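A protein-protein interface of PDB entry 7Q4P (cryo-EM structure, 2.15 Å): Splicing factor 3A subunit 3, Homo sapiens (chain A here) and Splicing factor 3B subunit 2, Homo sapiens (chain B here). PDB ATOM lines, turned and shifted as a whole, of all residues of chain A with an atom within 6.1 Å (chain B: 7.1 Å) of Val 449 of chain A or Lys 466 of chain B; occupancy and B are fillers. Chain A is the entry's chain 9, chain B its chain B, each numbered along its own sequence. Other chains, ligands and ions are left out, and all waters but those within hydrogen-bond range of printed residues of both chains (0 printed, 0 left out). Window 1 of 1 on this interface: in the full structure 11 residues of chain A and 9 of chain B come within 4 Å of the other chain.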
ATOM      1  N   CYS A 408     -15.504 -13.169 -34.093  1.00  0.00           N
ATOM      2  CA  CYS A 408     -15.840 -13.255 -32.680  1.00  0.00           C
ATOM      3  C   CYS A 408     -17.347 -13.159 -32.500  1.00  0.00           C
ATOM      4  O   CYS A 408     -17.923 -12.188 -32.943  1.00  0.00           O
ATOM      5  CB  CYS A 408     -15.235 -12.091 -31.910  1.00  0.00           C
ATOM      6  SG  CYS A 408     -15.287 -12.335 -30.117  1.00  0.00           S
ATOM      7  N   ILE A 410     -18.842 -13.042 -29.542  1.00  0.00           N
ATOM      8  CA  ILE A 410     -19.100 -12.189 -28.393  1.00  0.00           C
ATOM      9  C   ILE A 410     -19.201 -10.755 -28.896  1.00  0.00           C
ATOM     10  O   ILE A 410     -19.684  -9.876 -28.188  1.00  0.00           O
ATOM     11  CB  ILE A 410     -17.978 -12.339 -27.347  1.00  0.00           C
ATOM     12  CG1 ILE A 410     -17.509 -13.782 -27.184  1.00  0.00           C
ATOM     13  CG2 ILE A 410     -18.331 -11.714 -26.002  1.00  0.00           C
ATOM     14  CD1 ILE A 410     -18.430 -14.631 -26.355  1.00  0.00           C
ATOM     15  N   HIS A 425      -8.202  -7.384 -29.473  1.00  0.00           N
ATOM     16  CA  HIS A 425      -9.576  -7.002 -29.187  1.00  0.00           C
ATOM     17  C   HIS A 425     -10.121  -7.559 -27.869  1.00  0.00           C
ATOM     18  O   HIS A 425     -11.007  -6.958 -27.268  1.00  0.00           O
ATOM     19  CB  HIS A 425     -10.467  -7.318 -30.380  1.00  0.00           C
ATOM     20  CG  HIS A 425     -10.923  -8.726 -30.484  1.00  0.00           C
ATOM     21  ND1 HIS A 425     -11.894  -9.305 -29.653  1.00  0.00           N
ATOM     22  CD2 HIS A 425     -10.593  -9.652 -31.392  1.00  0.00           C
ATOM     23  CE1 HIS A 425     -12.062 -10.549 -30.041  1.00  0.00           C
ATOM     24  NE2 HIS A 425     -11.298 -10.768 -31.095  1.00  0.00           N
ATOM     25  N   PHE A 426      -9.650  -8.747 -27.466  1.00  0.00           N
ATOM     26  CA  PHE A 426     -10.134  -9.377 -26.248  1.00  0.00           C
ATOM     27  C   PHE A 426      -9.971  -8.475 -25.021  1.00  0.00           C
ATOM     28  O   PHE A 426     -10.494  -8.787 -23.951  1.00  0.00           O
ATOM     29  CB  PHE A 426      -9.486 -10.748 -26.069  1.00  0.00           C
ATOM     30  CG  PHE A 426      -9.854 -11.724 -27.147  1.00  0.00           C
ATOM     31  CD1 PHE A 426     -11.057 -12.396 -27.082  1.00  0.00           C
ATOM     32  CD2 PHE A 426      -8.957 -12.033 -28.152  1.00  0.00           C
ATOM     33  CE1 PHE A 426     -11.399 -13.326 -28.043  1.00  0.00           C
ATOM     34  CE2 PHE A 426      -9.294 -12.969 -29.115  1.00  0.00           C
ATOM     35  CZ  PHE A 426     -10.515 -13.609 -29.060  1.00  0.00           C
ATOM     36  N   HIS A 431     -15.425  -6.362 -27.159  1.00  0.00           N
ATOM     37  CA  HIS A 431     -15.411  -7.687 -26.578  1.00  0.00           C
ATOM     38  C   HIS A 431     -15.868  -7.595 -25.130  1.00  0.00           C
ATOM     39  O   HIS A 431     -16.604  -8.475 -24.690  1.00  0.00           O
ATOM     40  CB  HIS A 431     -14.045  -8.365 -26.734  1.00  0.00           C
ATOM     41  CG  HIS A 431     -14.104  -9.806 -26.356  1.00  0.00           C
ATOM     42  ND1 HIS A 431     -14.646 -10.805 -27.167  1.00  0.00           N
ATOM     43  CD2 HIS A 431     -13.773 -10.402 -25.193  1.00  0.00           C
ATOM     44  CE1 HIS A 431     -14.571 -11.962 -26.528  1.00  0.00           C
ATOM     45  NE2 HIS A 431     -14.058 -11.737 -25.304  1.00  0.00           N
ATOM     46  N   MET A 435     -19.014  -9.316 -23.229  1.00  0.00           N
ATOM     47  CA  MET A 435     -18.802 -10.136 -22.059  1.00  0.00           C
ATOM     48  C   MET A 435     -19.655  -9.615 -20.908  1.00  0.00           C
ATOM     49  O   MET A 435     -20.099 -10.429 -20.112  1.00  0.00           O
ATOM     50  CB  MET A 435     -17.324 -10.125 -21.683  1.00  0.00           C
ATOM     51  CG  MET A 435     -16.487 -10.977 -22.614  1.00  0.00           C
ATOM     52  SD  MET A 435     -16.636 -12.749 -22.356  1.00  0.00           S
ATOM     53  CE  MET A 435     -15.674 -12.881 -20.849  1.00  0.00           C
ATOM     54  N   ALA A 444      -8.245 -12.932 -18.443  1.00  0.00           N
ATOM     55  CA  ALA A 444      -7.280 -13.532 -19.353  1.00  0.00           C
ATOM     56  C   ALA A 444      -7.674 -14.982 -19.626  1.00  0.00           C
ATOM     57  O   ALA A 444      -7.169 -15.606 -20.563  1.00  0.00           O
ATOM     58  CB  ALA A 444      -5.888 -13.428 -18.779  1.00  0.00           C
ATOM     59  N   HIS A 445      -8.577 -15.485 -18.773  1.00  0.00           N
ATOM     60  CA  HIS A 445      -9.173 -16.800 -18.924  1.00  0.00           C
ATOM     61  C   HIS A 445      -9.944 -16.922 -20.234  1.00  0.00           C
ATOM     62  O   HIS A 445      -9.955 -17.998 -20.828  1.00  0.00           O
ATOM     63  CB  HIS A 445     -10.103 -17.083 -17.745  1.00  0.00           C
ATOM     64  CG  HIS A 445      -9.382 -17.225 -16.450  1.00  0.00           C
ATOM     65  ND1 HIS A 445      -9.169 -16.157 -15.596  1.00  0.00           N
ATOM     66  CD2 HIS A 445      -8.842 -18.305 -15.853  1.00  0.00           C
ATOM     67  CE1 HIS A 445      -8.519 -16.573 -14.528  1.00  0.00           C
ATOM     68  NE2 HIS A 445      -8.310 -17.893 -14.660  1.00  0.00           N
ATOM     69  N   PHE A 446     -10.588 -15.830 -20.668  1.00  0.00           N
ATOM     70  CA  PHE A 446     -11.528 -15.905 -21.775  1.00  0.00           C
ATOM     71  C   PHE A 446     -10.973 -15.213 -23.008  1.00  0.00           C
ATOM     72  O   PHE A 446     -11.729 -14.864 -23.911  1.00  0.00           O
ATOM     73  CB  PHE A 446     -12.812 -15.182 -21.382  1.00  0.00           C
ATOM     74  CG  PHE A 446     -13.486 -15.810 -20.202  1.00  0.00           C
ATOM     75  CD1 PHE A 446     -14.332 -16.904 -20.362  1.00  0.00           C
ATOM     76  CD2 PHE A 446     -13.269 -15.298 -18.931  1.00  0.00           C
ATOM     77  CE1 PHE A 446     -14.943 -17.492 -19.266  1.00  0.00           C
ATOM     78  CE2 PHE A 446     -13.881 -15.888 -17.839  1.00  0.00           C
ATOM     79  CZ  PHE A 446     -14.706 -16.985 -18.006  1.00  0.00           C
ATOM     80  N   ALA A 447      -9.668 -14.927 -22.991  1.00  0.00           N
ATOM     81  CA  ALA A 447      -9.005 -14.500 -24.211  1.00  0.00           C
ATOM     82  C   ALA A 447      -8.951 -15.679 -25.173  1.00  0.00           C
ATOM     83  O   ALA A 447      -8.732 -16.820 -24.759  1.00  0.00           O
ATOM     84  CB  ALA A 447      -7.620 -14.004 -23.907  1.00  0.00           C
ATOM     85  N   ASN A 448      -9.127 -15.359 -26.456  1.00  0.00           N
ATOM     86  CA  ASN A 448      -9.083 -16.343 -27.532  1.00  0.00           C
ATOM     87  C   ASN A 448     -10.332 -17.227 -27.484  1.00  0.00           C
ATOM     88  O   ASN A 448     -10.368 -18.309 -28.054  1.00  0.00           O
ATOM     89  CB  ASN A 448      -7.744 -17.087 -27.593  1.00  0.00           C
ATOM     90  CG  ASN A 448      -6.553 -16.163 -27.756  1.00  0.00           C
ATOM     91  OD1 ASN A 448      -6.455 -15.438 -28.748  1.00  0.00           O
ATOM     92  ND2 ASN A 448      -5.636 -16.189 -26.799  1.00  0.00           N
ATOM     93  N   VAL A 449     -11.372 -16.739 -26.809  1.00  0.00           N
ATOM     94  CA  VAL A 449     -12.639 -17.427 -26.744  1.00  0.00           C
ATOM     95  C   VAL A 449     -13.662 -16.536 -27.440  1.00  0.00           C
ATOM     96  O   VAL A 449     -13.923 -15.414 -27.017  1.00  0.00           O
ATOM     97  CB  VAL A 449     -13.044 -17.750 -25.299  1.00  0.00           C
ATOM     98  CG1 VAL A 449     -14.370 -18.454 -25.345  1.00  0.00           C
ATOM     99  CG2 VAL A 449     -12.034 -18.611 -24.545  1.00  0.00           C
ATOM    100  N   THR A 450     -14.195 -17.046 -28.548  1.00  0.00           N
ATOM    101  CA  THR A 450     -14.912 -16.233 -29.508  1.00  0.00           C
ATOM    102  C   THR A 450     -16.363 -16.667 -29.495  1.00  0.00           C
ATOM    103  O   THR A 450     -17.244 -15.836 -29.624  1.00  0.00           O
ATOM    104  CB  THR A 450     -14.342 -16.435 -30.914  1.00  0.00           C
ATOM    105  OG1 THR A 450     -14.166 -17.819 -31.204  1.00  0.00           O
ATOM    106  CG2 THR A 450     -13.024 -15.730 -31.091  1.00  0.00           C
ATOM    107  N   GLN A 451     -16.606 -17.969 -29.320  1.00  0.00           N
ATOM    108  CA  GLN A 451     -17.959 -18.491 -29.299  1.00  0.00           C
ATOM    109  C   GLN A 451     -18.587 -18.198 -27.943  1.00  0.00           C
ATOM    110  O   GLN A 451     -17.889 -18.100 -26.930  1.00  0.00           O
ATOM    111  CB  GLN A 451     -17.988 -19.953 -29.724  1.00  0.00           C
ATOM    112  CG  GLN A 451     -17.670 -20.131 -31.199  1.00  0.00           C
ATOM    113  CD  GLN A 451     -17.624 -21.584 -31.603  1.00  0.00           C
ATOM    114  OE1 GLN A 451     -16.849 -22.377 -31.074  1.00  0.00           O
ATOM    115  NE2 GLN A 451     -18.456 -21.940 -32.569  1.00  0.00           N
ATOM    116  N   ASP A 454     -19.065 -21.472 -25.462  1.00  0.00           N
ATOM    117  CA  ASP A 454     -17.817 -21.871 -24.840  1.00  0.00           C
ATOM    118  C   ASP A 454     -17.478 -20.938 -23.683  1.00  0.00           C
ATOM    119  O   ASP A 454     -17.073 -21.397 -22.611  1.00  0.00           O
ATOM    120  CB  ASP A 454     -16.667 -21.895 -25.840  1.00  0.00           C
ATOM    121  CG  ASP A 454     -15.439 -22.503 -25.196  1.00  0.00           C
ATOM    122  OD1 ASP A 454     -15.397 -23.745 -25.086  1.00  0.00           O
ATOM    123  OD2 ASP A 454     -14.564 -21.728 -24.753  1.00  0.00           O
ATOM    124  N   ALA A 455     -17.711 -19.638 -23.890  1.00  0.00           N
ATOM    125  CA  ALA A 455     -17.422 -18.659 -22.856  1.00  0.00           C
ATOM    126  C   ALA A 455     -18.342 -18.832 -21.655  1.00  0.00           C
ATOM    127  O   ALA A 455     -17.964 -18.413 -20.575  1.00  0.00           O
ATOM    128  CB  ALA A 455     -17.520 -17.246 -23.353  1.00  0.00           C
ATOM    129  N   LEU A 458     -17.070 -22.166 -19.848  1.00  0.00           N
ATOM    130  CA  LEU A 458     -15.800 -21.921 -19.201  1.00  0.00           C
ATOM    131  C   LEU A 458     -16.038 -21.084 -17.950  1.00  0.00           C
ATOM    132  O   LEU A 458     -15.315 -21.233 -16.972  1.00  0.00           O
ATOM    133  CB  LEU A 458     -14.875 -21.206 -20.185  1.00  0.00           C
ATOM    134  CG  LEU A 458     -13.393 -21.160 -19.818  1.00  0.00           C
ATOM    135  CD1 LEU A 458     -12.757 -22.544 -19.929  1.00  0.00           C
ATOM    136  CD2 LEU A 458     -12.674 -20.197 -20.748  1.00  0.00           C
ATOM    137  N   LYS A 461     -17.242 -23.315 -15.316  1.00  0.00           N
ATOM    138  CA  LYS A 461     -16.185 -24.161 -14.795  1.00  0.00           C
ATOM    139  C   LYS A 461     -15.363 -23.377 -13.780  1.00  0.00           C
ATOM    140  O   LYS A 461     -15.036 -23.928 -12.740  1.00  0.00           O
ATOM    141  CB  LYS A 461     -15.251 -24.679 -15.897  1.00  0.00           C
ATOM    142  CG  LYS A 461     -14.511 -25.965 -15.554  1.00  0.00           C
ATOM    143  CD  LYS A 461     -13.285 -26.237 -16.428  1.00  0.00           C
ATOM    144  CE  LYS A 461     -12.109 -25.321 -16.142  1.00  0.00           C
ATOM    145  NZ  LYS A 461     -10.938 -25.629 -16.996  1.00  0.00           N
ATOM    146  N   PHE B 460      -6.949 -29.693 -30.566  1.00  0.00           N
ATOM    147  CA  PHE B 460      -7.954 -29.028 -29.745  1.00  0.00           C
ATOM    148  C   PHE B 460      -8.227 -27.639 -30.325  1.00  0.00           C
ATOM    149  O   PHE B 460      -7.366 -27.063 -30.975  1.00  0.00           O
ATOM    150  CB  PHE B 460      -7.468 -28.829 -28.300  1.00  0.00           C
ATOM    151  CG  PHE B 460      -6.986 -30.060 -27.553  1.00  0.00           C
ATOM    152  CD1 PHE B 460      -7.857 -31.102 -27.241  1.00  0.00           C
ATOM    153  CD2 PHE B 460      -5.664 -30.166 -27.118  1.00  0.00           C
ATOM    154  CE1 PHE B 460      -7.406 -32.223 -26.549  1.00  0.00           C
ATOM    155  CE2 PHE B 460      -5.215 -31.285 -26.425  1.00  0.00           C
ATOM    156  CZ  PHE B 460      -6.091 -32.311 -26.141  1.00  0.00           C
ATOM    157  N   THR B 461      -9.406 -27.078 -30.050  1.00  0.00           N
ATOM    158  CA  THR B 461      -9.603 -25.649 -30.178  1.00  0.00           C
ATOM    159  C   THR B 461      -9.118 -25.003 -28.885  1.00  0.00           C
ATOM    160  O   THR B 461      -8.995 -25.673 -27.857  1.00  0.00           O
ATOM    161  CB  THR B 461     -11.064 -25.297 -30.485  1.00  0.00           C
ATOM    162  OG1 THR B 461     -11.946 -25.884 -29.526  1.00  0.00           O
ATOM    163  CG2 THR B 461     -11.491 -25.714 -31.876  1.00  0.00           C
ATOM    164  N   VAL B 462      -8.895 -23.699 -28.932  1.00  0.00           N
ATOM    165  CA  VAL B 462      -8.451 -22.989 -27.746  1.00  0.00           C
ATOM    166  C   VAL B 462      -9.557 -23.054 -26.704  1.00  0.00           C
ATOM    167  O   VAL B 462      -9.281 -22.863 -25.540  1.00  0.00           O
ATOM    168  CB  VAL B 462      -8.073 -21.531 -28.056  1.00  0.00           C
ATOM    169  CG1 VAL B 462      -7.638 -20.760 -26.811  1.00  0.00           C
ATOM    170  CG2 VAL B 462      -6.998 -21.467 -29.117  1.00  0.00           C
ATOM    171  N   ALA B 463     -10.796 -23.172 -27.176  1.00  0.00           N
ATOM    172  CA  ALA B 463     -11.977 -23.248 -26.342  1.00  0.00           C
ATOM    173  C   ALA B 463     -11.961 -24.592 -25.622  1.00  0.00           C
ATOM    174  O   ALA B 463     -12.357 -24.646 -24.467  1.00  0.00           O
ATOM    175  CB  ALA B 463     -13.179 -23.127 -27.243  1.00  0.00           C
ATOM    176  N   GLU B 464     -11.551 -25.650 -26.337  1.00  0.00           N
ATOM    177  CA  GLU B 464     -11.612 -27.023 -25.864  1.00  0.00           C
ATOM    178  C   GLU B 464     -10.479 -27.316 -24.877  1.00  0.00           C
ATOM    179  O   GLU B 464     -10.703 -27.959 -23.848  1.00  0.00           O
ATOM    180  CB  GLU B 464     -11.611 -27.946 -27.080  1.00  0.00           C
ATOM    181  CG  GLU B 464     -11.973 -29.388 -26.792  1.00  0.00           C
ATOM    182  CD  GLU B 464     -11.791 -30.364 -27.947  1.00  0.00           C
ATOM    183  OE1 GLU B 464     -12.165 -30.007 -29.086  1.00  0.00           O
ATOM    184  OE2 GLU B 464     -11.294 -31.490 -27.708  1.00  0.00           O
ATOM    185  N   LEU B 465      -9.281 -26.773 -25.148  1.00  0.00           N
ATOM    186  CA  LEU B 465      -8.123 -26.896 -24.266  1.00  0.00           C
ATOM    187  C   LEU B 465      -8.325 -26.179 -22.921  1.00  0.00           C
ATOM    188  O   LEU B 465      -7.931 -26.703 -21.883  1.00  0.00           O
ATOM    189  CB  LEU B 465      -6.878 -26.414 -25.021  1.00  0.00           C
ATOM    190  CG  LEU B 465      -5.547 -26.506 -24.270  1.00  0.00           C
ATOM    191  CD1 LEU B 465      -5.239 -27.927 -23.811  1.00  0.00           C
ATOM    192  CD2 LEU B 465      -4.412 -26.004 -25.142  1.00  0.00           C
ATOM    193  N   LYS B 466      -8.970 -25.006 -22.906  1.00  0.00           N
ATOM    194  CA  LYS B 466      -9.194 -24.244 -21.684  1.00  0.00           C
ATOM    195  C   LYS B 466     -10.146 -24.967 -20.739  1.00  0.00           C
ATOM    196  O   LYS B 466     -10.090 -24.738 -19.535  1.00  0.00           O
ATOM    197  CB  LYS B 466      -9.739 -22.857 -22.014  1.00  0.00           C
ATOM    198  CG  LYS B 466      -8.683 -21.888 -22.507  1.00  0.00           C
ATOM    199  CD  LYS B 466      -9.260 -20.540 -22.826  1.00  0.00           C
ATOM    200  CE  LYS B 466      -8.217 -19.621 -23.416  1.00  0.00           C
ATOM    201  NZ  LYS B 466      -7.654 -18.691 -22.409  1.00  0.00           N
ATOM    202  N   GLN B 467     -10.986 -25.858 -21.274  1.00  0.00           N
ATOM    203  CA  GLN B 467     -11.900 -26.634 -20.453  1.00  0.00           C
ATOM    204  C   GLN B 467     -11.158 -27.774 -19.765  1.00  0.00           C
ATOM    205  O   GLN B 467     -11.549 -28.179 -18.675  1.00  0.00           O
ATOM    206  CB  GLN B 467     -12.970 -27.302 -21.313  1.00  0.00           C
ATOM    207  CG  GLN B 467     -13.920 -26.315 -21.954  1.00  0.00           C
ATOM    208  CD  GLN B 467     -14.966 -25.782 -21.003  1.00  0.00           C
ATOM    209  OE1 GLN B 467     -15.325 -26.412 -20.010  1.00  0.00           O
ATOM    210  NE2 GLN B 467     -15.475 -24.603 -21.311  1.00  0.00           N
ATOM    211  N   LEU B 468     -10.097 -28.290 -20.411  1.00  0.00           N
ATOM    212  CA  LEU B 468      -9.358 -29.492 -20.021  1.00  0.00           C
ATOM    213  C   LEU B 468      -8.196 -29.220 -19.051  1.00  0.00           C
ATOM    214  O   LEU B 468      -7.601 -30.168 -18.529  1.00  0.00           O
ATOM    215  CB  LEU B 468      -8.843 -30.199 -21.288  1.00  0.00           C
ATOM    216  CG  LEU B 468      -9.891 -30.833 -22.204  1.00  0.00           C
ATOM    217  CD1 LEU B 468      -9.269 -31.211 -23.543  1.00  0.00           C
ATOM    218  CD2 LEU B 468     -10.527 -32.059 -21.559  1.00  0.00           C
ATOM    219  N   VAL B 469      -7.845 -27.943 -18.810  1.00  0.00           N
ATOM    220  CA  VAL B 469      -6.657 -27.566 -18.045  1.00  0.00           C
ATOM    221  C   VAL B 469      -7.008 -26.806 -16.762  1.00  0.00           C
ATOM    222  O   VAL B 469      -8.022 -26.109 -16.686  1.00  0.00           O
ATOM    223  CB  VAL B 469      -5.651 -26.768 -18.902  1.00  0.00           C
ATOM    224  CG1 VAL B 469      -5.160 -27.589 -20.083  1.00  0.00           C
ATOM    225  CG2 VAL B 469      -6.213 -25.427 -19.361  1.00  0.00           C
ATOM    226  N   ALA B 470      -6.102 -26.907 -15.777  1.00  0.00           N
ATOM    227  CA  ALA B 470      -6.251 -26.283 -14.463  1.00  0.00           C
ATOM    228  C   ALA B 470      -5.996 -24.770 -14.495  1.00  0.00           C
ATOM    229  O   ALA B 470      -6.497 -24.024 -13.647  1.00  0.00           O
ATOM    230  CB  ALA B 470      -5.359 -26.975 -13.463  1.00  0.00           C
ATOM    231  N   ARG B 471      -5.250 -24.291 -15.515  1.00  0.00           N
ATOM    232  CA  ARG B 471      -4.920 -22.872 -15.667  1.00  0.00           C
ATOM    233  C   ARG B 471      -5.353 -22.395 -17.061  1.00  0.00           C
ATOM    234  O   ARG B 471      -4.521 -22.110 -17.911  1.00  0.00           O
ATOM    235  CB  ARG B 471      -3.431 -22.651 -15.369  1.00  0.00           C
ATOM    236  CG  ARG B 471      -3.097 -21.204 -15.075  1.00  0.00           C
ATOM    237  CD  ARG B 471      -1.670 -21.015 -14.638  1.00  0.00           C
ATOM    238  NE  ARG B 471      -1.147 -19.735 -14.228  1.00  0.00           N
ATOM    239  CZ  ARG B 471      -1.711 -18.751 -13.552  1.00  0.00           C
ATOM    240  NH1 ARG B 471      -3.020 -18.690 -13.348  1.00  0.00           N
ATOM    241  NH2 ARG B 471      -0.958 -17.715 -13.264  1.00  0.00           N
ATOM    242  N   PRO B 472      -6.671 -22.155 -17.281  1.00  0.00           N
ATOM    243  CA  PRO B 472      -7.167 -21.708 -18.582  1.00  0.00           C
ATOM    244  C   PRO B 472      -6.574 -20.378 -19.056  1.00  0.00           C
ATOM    245  O   PRO B 472      -6.527 -20.128 -20.249  1.00  0.00           O
ATOM    246  CB  PRO B 472      -8.684 -21.550 -18.374  1.00  0.00           C
ATOM    247  CG  PRO B 472      -8.992 -22.446 -17.195  1.00  0.00           C
ATOM    248  CD  PRO B 472      -7.765 -22.343 -16.316  1.00  0.00           C
ATOM    249  N   ASP B 473      -6.109 -19.507 -18.141  1.00  0.00           N
ATOM    250  CA  ASP B 473      -5.635 -18.174 -18.534  1.00  0.00           C
ATOM    251  C   ASP B 473      -4.266 -18.197 -19.229  1.00  0.00           C
ATOM    252  O   ASP B 473      -4.052 -17.400 -20.145  1.00  0.00           O
ATOM    253  CB  ASP B 473      -5.665 -17.152 -17.392  1.00  0.00           C
ATOM    254  CG  ASP B 473      -4.853 -17.561 -16.175  1.00  0.00           C
ATOM    255  OD1 ASP B 473      -5.486 -17.908 -15.164  1.00  0.00           O
ATOM    256  OD2 ASP B 473      -3.610 -17.493 -16.236  1.00  0.00           O
ATOM    257  N   VAL B 474      -3.332 -19.065 -18.785  1.00  0.00           N
ATOM    258  CA  VAL B 474      -2.033 -19.188 -19.447  1.00  0.00           C
ATOM    259  C   VAL B 474      -2.233 -19.640 -20.889  1.00  0.00           C
ATOM    260  O   VAL B 474      -1.472 -19.208 -21.754  1.00  0.00           O
ATOM    261  CB  VAL B 474      -0.983 -20.068 -18.724  1.00  0.00           C
ATOM    262  CG1 VAL B 474      -0.460 -19.438 -17.451  1.00  0.00           C
ATOM    263  CG2 VAL B 474      -1.437 -21.498 -18.477  1.00  0.00           C
ATOM    264  N   VAL B 475      -3.278 -20.459 -21.144  1.00  0.00           N
ATOM    265  CA  VAL B 475      -3.499 -21.017 -22.486  1.00  0.00           C
ATOM    266  C   VAL B 475      -3.462 -19.866 -23.488  1.00  0.00           C
ATOM    267  O   VAL B 475      -4.135 -18.866 -23.248  1.00  0.00           O
ATOM    268  CB  VAL B 475      -4.834 -21.785 -22.635  1.00  0.00           C
ATOM    269  CG1 VAL B 475      -5.070 -22.266 -24.064  1.00  0.00           C
ATOM    270  CG2 VAL B 475      -4.957 -22.956 -21.678  1.00  0.00           C
ATOM    271  N   GLU B 476      -2.662 -20.014 -24.558  1.00  0.00           N
ATOM    272  CA  GLU B 476      -2.473 -18.992 -25.580  1.00  0.00           C
ATOM    273  C   GLU B 476      -3.030 -19.547 -26.889  1.00  0.00           C
ATOM    274  O   GLU B 476      -3.411 -20.715 -26.926  1.00  0.00           O
ATOM    275  CB  GLU B 476      -0.997 -18.588 -25.661  1.00  0.00           C
ATOM    276  CG  GLU B 476      -0.637 -17.471 -24.695  1.00  0.00           C
ATOM    277  CD  GLU B 476       0.675 -16.754 -24.950  1.00  0.00           C
ATOM    278  OE1 GLU B 476       0.671 -15.780 -25.729  1.00  0.00           O
ATOM    279  OE2 GLU B 476       1.696 -17.158 -24.358  1.00  0.00           O
ATOM    280  N   MET B 477      -3.081 -18.716 -27.942  1.00  0.00           N
ATOM    281  CA  MET B 477      -3.707 -19.116 -29.197  1.00  0.00           C
ATOM    282  C   MET B 477      -2.902 -20.200 -29.919  1.00  0.00           C
ATOM    283  O   MET B 477      -3.489 -21.094 -30.514  1.00  0.00           O
ATOM    284  CB  MET B 477      -3.894 -17.920 -30.135  1.00  0.00           C
ATOM    285  CG  MET B 477      -4.999 -18.136 -31.153  1.00  0.00           C
ATOM    286  SD  MET B 477      -5.249 -16.754 -32.298  1.00  0.00           S
ATOM    287  CE  MET B 477      -3.769 -16.875 -33.302  1.00  0.00           C
ATOM    288  N   VAL B 480      -2.478 -24.666 -28.887  1.00  0.00           N
ATOM    289  CA  VAL B 480      -3.190 -25.832 -29.412  1.00  0.00           C
ATOM    290  C   VAL B 480      -2.449 -26.448 -30.600  1.00  0.00           C
ATOM    291  O   VAL B 480      -2.769 -27.543 -31.043  1.00  0.00           O
ATOM    292  CB  VAL B 480      -4.644 -25.492 -29.792  1.00  0.00           C
ATOM    293  CG1 VAL B 480      -5.455 -25.206 -28.553  1.00  0.00           C
ATOM    294  CG2 VAL B 480      -4.737 -24.328 -30.769  1.00  0.00           C
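The backbone carbonyl oxygen of His 445 of chain A is in hydrogen-bond range of the side-chain amino group of Lys 466 of chain B.
O of Ala 447 of chain A sits close to NZ of Lys 466 of chain B (3.2 Å).
OD1 of Asp 454 of chain A lies close to O of Ala 463 of chain B (3.2 Å).
O of Lys 466 of chain B is in hydrogen-bond range of NZ of Lys 461 of chain A (2.8 Å).
The side-chain amino group (NZ) of Lys 461 of chain A is in hydrogen-bond range of the backbone carbonyl oxygen (O) of Val 469 of chain B (3.0 Å).
The side-chain amino group (NZ) of Lys 461 of chain A sits at hydrogen-bond distance from the backbone carbonyl oxygen (O) of Gln 467 of chain B, at 3.1 Å.
The backbone NH of Leu 458 of chain A sits close to the side-chain amide nitrogen of Gln 467 of chain B (3.3 Å).
NE2 of His 445 of chain A sits at hydrogen-bond distance from OD1 of Asp 473 of chain B.
The side-chain amino group of Lys 466 of chain B lies within hydrogen-bond range of the backbone carbonyl oxygen of Pro 472 of chain B (2.8 Å).
The guanidinium group (NH1) of Arg 471 of chain B is in salt-bridge range of the side-chain carboxylate (OD1) of Asp 473 of chain B, 3.2 Å away.
Among the printed residues, pairs that only touch across the chains: Leu 458 of chain A with Lys 466 of chain B, Ala 444 of chain A with Asp 473 of chain B, Ala 444 of chain A with Lys 466 of chain B, Lys 461 of chain A with Pro 472 of chain B, Asn 448 of chain A with Val 462 of chain B, Asn 448 of chain A with Met 477 of chain B, Val 449 of chain A with Lys 466 of chain B and Asp 454 of chain A with Gln 467 of chain B.
Val 449 of chain A touches just one residue of chain B: Lys 466.
Of chain A, only Ala 444, His 445, Ala 447, Val 449, Leu 458 and Lys 461 come within 4 Å of Lys 466 of chain B.
Printed residues of chain B within 4 Å of Lys 461 of chain A: Lys 466 (2.8 Å), Gln 467 (3.1 Å), Val 469 (3.0 Å) and Pro 472 (3.7 Å).
Of the printed residues of chain B, Leu 458 of chain A touches Lys 466 (3.5 Å) and Gln 467 (3.3 Å).
The nearest printed residue of chain B that does not touch His 445 of chain A is Pro 472 of chain B (4.1 Å).
Of the 18 printed residues of chain A, 8 touch a printed residue of chain B.
Among the printed residues, 16 pairs touch across the chains.
Among the printed residues, no Asp or Glu carboxylate lies within 4 Å of a Lys or Arg side-chain nitrogen of the other chain.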
